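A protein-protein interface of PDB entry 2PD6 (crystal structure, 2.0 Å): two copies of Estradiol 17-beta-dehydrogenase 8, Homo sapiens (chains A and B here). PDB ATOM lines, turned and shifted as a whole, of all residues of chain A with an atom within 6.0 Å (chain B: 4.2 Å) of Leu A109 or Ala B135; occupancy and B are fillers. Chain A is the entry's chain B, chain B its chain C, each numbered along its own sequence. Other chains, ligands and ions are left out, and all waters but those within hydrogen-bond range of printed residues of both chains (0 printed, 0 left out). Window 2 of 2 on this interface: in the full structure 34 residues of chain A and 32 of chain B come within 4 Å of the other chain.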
ATOM      1  N   PHE A 107       3.341 -22.711 -31.418  1.00  0.00           N
ATOM      2  CA  PHE A 107       3.830 -21.779 -30.394  1.00  0.00           C
ATOM      3  C   PHE A 107       2.720 -20.867 -29.877  1.00  0.00           C
ATOM      4  O   PHE A 107       1.876 -20.392 -30.652  1.00  0.00           O
ATOM      5  CB  PHE A 107       4.954 -20.916 -30.934  1.00  0.00           C
ATOM      6  CG  PHE A 107       6.228 -21.661 -31.166  1.00  0.00           C
ATOM      7  CD1 PHE A 107       6.822 -21.673 -32.422  1.00  0.00           C
ATOM      8  CD2 PHE A 107       6.838 -22.353 -30.130  1.00  0.00           C
ATOM      9  CE1 PHE A 107       8.015 -22.351 -32.637  1.00  0.00           C
ATOM     10  CE2 PHE A 107       8.025 -23.045 -30.342  1.00  0.00           C
ATOM     11  CZ  PHE A 107       8.611 -23.042 -31.595  1.00  0.00           C
ATOM     12  N   LEU A 108       2.752 -20.598 -28.571  1.00  0.00           N
ATOM     13  CA  LEU A 108       1.757 -19.732 -27.936  1.00  0.00           C
ATOM     14  C   LEU A 108       1.554 -18.418 -28.700  1.00  0.00           C
ATOM     15  O   LEU A 108       0.430 -17.939 -28.841  1.00  0.00           O
ATOM     16  CB  LEU A 108       2.155 -19.415 -26.487  1.00  0.00           C
ATOM     17  CG  LEU A 108       1.308 -18.360 -25.759  1.00  0.00           C
ATOM     18  CD1 LEU A 108      -0.085 -18.916 -25.478  1.00  0.00           C
ATOM     19  CD2 LEU A 108       1.984 -17.902 -24.457  1.00  0.00           C
ATOM     20  N   LEU A 109       2.645 -17.844 -29.194  1.00  0.00           N
ATOM     21  CA  LEU A 109       2.573 -16.555 -29.881  1.00  0.00           C
ATOM     22  C   LEU A 109       1.807 -16.602 -31.202  1.00  0.00           C
ATOM     23  O   LEU A 109       1.426 -15.545 -31.719  1.00  0.00           O
ATOM     24  CB  LEU A 109       3.978 -15.993 -30.168  1.00  0.00           C
ATOM     25  CG  LEU A 109       4.781 -15.481 -28.976  1.00  0.00           C
ATOM     26  CD1 LEU A 109       6.211 -15.176 -29.395  1.00  0.00           C
ATOM     27  CD2 LEU A 109       4.120 -14.246 -28.331  1.00  0.00           C
ATOM     28  N   HIS A 110       1.642 -17.791 -31.773  1.00  0.00           N
ATOM     29  CA  HIS A 110       1.003 -17.926 -33.087  1.00  0.00           C
ATOM     30  C   HIS A 110      -0.247 -18.800 -33.055  1.00  0.00           C
ATOM     31  O   HIS A 110      -0.847 -19.039 -34.098  1.00  0.00           O
ATOM     32  CB  HIS A 110       1.993 -18.486 -34.126  1.00  0.00           C
ATOM     33  CG  HIS A 110       3.253 -17.688 -34.255  1.00  0.00           C
ATOM     34  ND1 HIS A 110       3.335 -16.532 -35.003  1.00  0.00           N
ATOM     35  CD2 HIS A 110       4.493 -17.904 -33.756  1.00  0.00           C
ATOM     36  CE1 HIS A 110       4.570 -16.064 -34.946  1.00  0.00           C
ATOM     37  NE2 HIS A 110       5.290 -16.875 -34.186  1.00  0.00           N
ATOM     38  N   MET A 111      -0.669 -19.230 -31.875  1.00  0.00           N
ATOM     39  CA  MET A 111      -1.704 -20.249 -31.775  1.00  0.00           C
ATOM     40  C   MET A 111      -3.108 -19.693 -32.014  1.00  0.00           C
ATOM     41  O   MET A 111      -3.546 -18.771 -31.330  1.00  0.00           O
ATOM     42  CB  MET A 111      -1.677 -20.901 -30.415  1.00  0.00           C
ATOM     43  CG  MET A 111      -2.718 -22.000 -30.293  1.00  0.00           C
ATOM     44  SD  MET A 111      -2.598 -22.892 -28.788  1.00  0.00           S
ATOM     45  CE  MET A 111      -1.098 -23.854 -29.034  1.00  0.00           C
ATOM     46  N   THR B 131      -2.832 -14.148 -21.541  1.00  0.00           N
ATOM     47  CA  THR B 131      -1.401 -14.549 -21.590  1.00  0.00           C
ATOM     48  C   THR B 131      -0.807 -14.402 -23.008  1.00  0.00           C
ATOM     49  O   THR B 131       0.302 -13.865 -23.182  1.00  0.00           O
ATOM     50  CB  THR B 131      -1.197 -15.987 -21.090  1.00  0.00           C
ATOM     51  OG1 THR B 131      -1.584 -16.093 -19.709  1.00  0.00           O
ATOM     52  CG2 THR B 131       0.260 -16.406 -21.215  1.00  0.00           C
ATOM     53  N   GLN B 132      -1.561 -14.847 -24.008  1.00  0.00           N
ATOM     54  CA  GLN B 132      -1.126 -14.775 -25.400  1.00  0.00           C
ATOM     55  C   GLN B 132      -1.089 -13.335 -25.880  1.00  0.00           C
ATOM     56  O   GLN B 132      -0.125 -12.920 -26.518  1.00  0.00           O
ATOM     57  CB  GLN B 132      -2.057 -15.588 -26.278  1.00  0.00           C
ATOM     58  CG  GLN B 132      -1.657 -15.680 -27.723  1.00  0.00           C
ATOM     59  CD  GLN B 132      -2.747 -16.256 -28.587  1.00  0.00           C
ATOM     60  OE1 GLN B 132      -3.916 -15.825 -28.503  1.00  0.00           O
ATOM     61  NE2 GLN B 132      -2.381 -17.219 -29.449  1.00  0.00           N
ATOM     62  N   ALA B 133      -2.149 -12.582 -25.589  1.00  0.00           N
ATOM     63  CA  ALA B 133      -2.259 -11.216 -26.093  1.00  0.00           C
ATOM     64  C   ALA B 133      -1.180 -10.358 -25.457  1.00  0.00           C
ATOM     65  O   ALA B 133      -0.535  -9.573 -26.137  1.00  0.00           O
ATOM     66  CB  ALA B 133      -3.653 -10.636 -25.834  1.00  0.00           C
ATOM     67  N   ALA B 134      -0.957 -10.549 -24.162  1.00  0.00           N
ATOM     68  CA  ALA B 134       0.090  -9.821 -23.439  1.00  0.00           C
ATOM     69  C   ALA B 134       1.490 -10.140 -23.977  1.00  0.00           C
ATOM     70  O   ALA B 134       2.289  -9.245 -24.231  1.00  0.00           O
ATOM     71  CB  ALA B 134       0.014 -10.115 -21.959  1.00  0.00           C
ATOM     72  N   ALA B 135       1.770 -11.421 -24.145  1.00  0.00           N
ATOM     73  CA  ALA B 135       3.055 -11.897 -24.666  1.00  0.00           C
ATOM     74  C   ALA B 135       3.336 -11.378 -26.070  1.00  0.00           C
ATOM     75  O   ALA B 135       4.455 -10.928 -26.363  1.00  0.00           O
ATOM     76  CB  ALA B 135       3.103 -13.457 -24.640  1.00  0.00           C
ATOM     77  N   GLN B 136       2.317 -11.426 -26.933  1.00  0.00           N
ATOM     78  CA  GLN B 136       2.445 -10.914 -28.299  1.00  0.00           C
ATOM     79  C   GLN B 136       2.895  -9.453 -28.281  1.00  0.00           C
ATOM     80  O   GLN B 136       3.800  -9.073 -29.031  1.00  0.00           O
ATOM     81  CB  GLN B 136       1.131 -11.101 -29.071  1.00  0.00           C
ATOM     82  CG  GLN B 136       0.864 -12.543 -29.554  1.00  0.00           C
ATOM     83  CD  GLN B 136      -0.554 -12.768 -30.124  1.00  0.00           C
ATOM     84  OE1 GLN B 136      -1.470 -11.988 -29.880  1.00  0.00           O
ATOM     85  NE2 GLN B 136      -0.727 -13.846 -30.878  1.00  0.00           N
ATOM     86  N   ALA B 137       2.280  -8.642 -27.414  1.00  0.00           N
ATOM     87  CA  ALA B 137       2.564  -7.193 -27.321  1.00  0.00           C
ATOM     88  C   ALA B 137       3.969  -6.945 -26.786  1.00  0.00           C
ATOM     89  O   ALA B 137       4.726  -6.125 -27.311  1.00  0.00           O
ATOM     90  CB  ALA B 137       1.554  -6.514 -26.412  1.00  0.00           C
ATOM     91  N   LEU B 138       4.316  -7.652 -25.725  1.00  0.00           N
ATOM     92  CA  LEU B 138       5.672  -7.590 -25.183  1.00  0.00           C
ATOM     93  C   LEU B 138       6.728  -7.985 -26.209  1.00  0.00           C
ATOM     94  O   LEU B 138       7.680  -7.231 -26.434  1.00  0.00           O
ATOM     95  CB  LEU B 138       5.793  -8.444 -23.918  1.00  0.00           C
ATOM     96  CG  LEU B 138       5.042  -7.840 -22.725  1.00  0.00           C
ATOM     97  CD1 LEU B 138       5.032  -8.790 -21.526  1.00  0.00           C
ATOM     98  CD2 LEU B 138       5.658  -6.495 -22.357  1.00  0.00           C
ATOM     99  N   VAL B 139       6.568  -9.131 -26.862  1.00  0.00           N
ATOM    100  CA  VAL B 139       7.605  -9.584 -27.817  1.00  0.00           C
ATOM    101  C   VAL B 139       7.739  -8.683 -29.034  1.00  0.00           C
ATOM    102  O   VAL B 139       8.863  -8.417 -29.499  1.00  0.00           O
ATOM    103  CB  VAL B 139       7.386 -11.050 -28.283  1.00  0.00           C
ATOM    104  CG1 VAL B 139       8.394 -11.440 -29.339  1.00  0.00           C
ATOM    105  CG2 VAL B 139       7.476 -12.003 -27.100  1.00  0.00           C
ATOM    106  N   LEU B 183       8.628 -18.636 -23.525  1.00  0.00           N
ATOM    107  CA  LEU B 183       8.785 -17.189 -23.465  1.00  0.00           C
ATOM    108  C   LEU B 183      10.034 -16.716 -22.698  1.00  0.00           C
ATOM    109  O   LEU B 183      10.404 -15.550 -22.782  1.00  0.00           O
ATOM    110  CB  LEU B 183       7.544 -16.570 -22.839  1.00  0.00           C
ATOM    111  CG  LEU B 183       6.238 -16.705 -23.598  1.00  0.00           C
ATOM    112  CD1 LEU B 183       5.150 -15.934 -22.832  1.00  0.00           C
ATOM    113  CD2 LEU B 183       6.393 -16.197 -25.048  1.00  0.00           C
ATOM    114  N   HIS B 186      12.514 -14.799 -24.572  1.00  0.00           N
ATOM    115  CA  HIS B 186      12.147 -13.433 -24.962  1.00  0.00           C
ATOM    116  C   HIS B 186      12.146 -12.509 -23.747  1.00  0.00           C
ATOM    117  O   HIS B 186      11.653 -11.378 -23.822  1.00  0.00           O
ATOM    118  CB  HIS B 186      10.749 -13.390 -25.596  1.00  0.00           C
ATOM    119  CG  HIS B 186      10.607 -14.205 -26.848  1.00  0.00           C
ATOM    120  ND1 HIS B 186      11.151 -13.821 -28.056  1.00  0.00           N
ATOM    121  CD2 HIS B 186       9.940 -15.360 -27.088  1.00  0.00           C
ATOM    122  CE1 HIS B 186      10.849 -14.719 -28.978  1.00  0.00           C
ATOM    123  NE2 HIS B 186      10.117 -15.664 -28.416  1.00  0.00           N
ATOM    124  N   ILE B 188      10.536 -12.992 -20.843  1.00  0.00           N
ATOM    125  CA  ILE B 188       9.214 -12.945 -20.215  1.00  0.00           C
ATOM    126  C   ILE B 188       9.061 -14.169 -19.288  1.00  0.00           C
ATOM    127  O   ILE B 188       9.235 -15.308 -19.706  1.00  0.00           O
ATOM    128  CB  ILE B 188       8.057 -12.897 -21.259  1.00  0.00           C
ATOM    129  CG1 ILE B 188       8.241 -11.737 -22.240  1.00  0.00           C
ATOM    130  CG2 ILE B 188       6.720 -12.733 -20.549  1.00  0.00           C
ATOM    131  CD1 ILE B 188       7.286 -11.751 -23.418  1.00  0.00           C
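No position is printed for both chains.
Leu A108 touches Thr B131. CD2 of Leu A109 touches C of Ala B135, at 3.7 Å.
Of the printed residues of chain A, Gln B136 touches Leu A109. Of the printed residues of chain B, Met A111 touches Gln B132. Ala B134 touches none of the printed residues of chain A. Val B139 touches none of the printed residues of chain A. The nearest residue of chain B that does not touch Leu A109 is His B186 (4.1 Å). The nearest residue of chain A that does not touch Ala B135 is Leu A108 (4.6 Å). The nearest printed residue of chain A that does not touch Gln B132 is His A110 (4.5 Å).
O of Leu A108 is in hydrogen-bond range of NE2 of Gln B132, at 3.0 Å. The backbone carbonyl oxygen of Leu A109 lies within hydrogen-bond range of the side-chain amide nitrogen of Gln B136, at 2.9 Å. O of Met A111 sits at hydrogen-bond distance from NE2 of Gln B132 (2.7 Å).
Printed residues of chain A that touch a printed residue of chain B: Leu A108, Leu A109 and Met A111. Hydrophobic or aromatic side chains of chain A within 4 Å of the printed part of chain B: Leu A108, Leu A109 and Met A111. Among the printed residues, no Asp or Glu carboxylate lies within 4 Å of a Lys or Arg side-chain nitrogen of the other chain.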
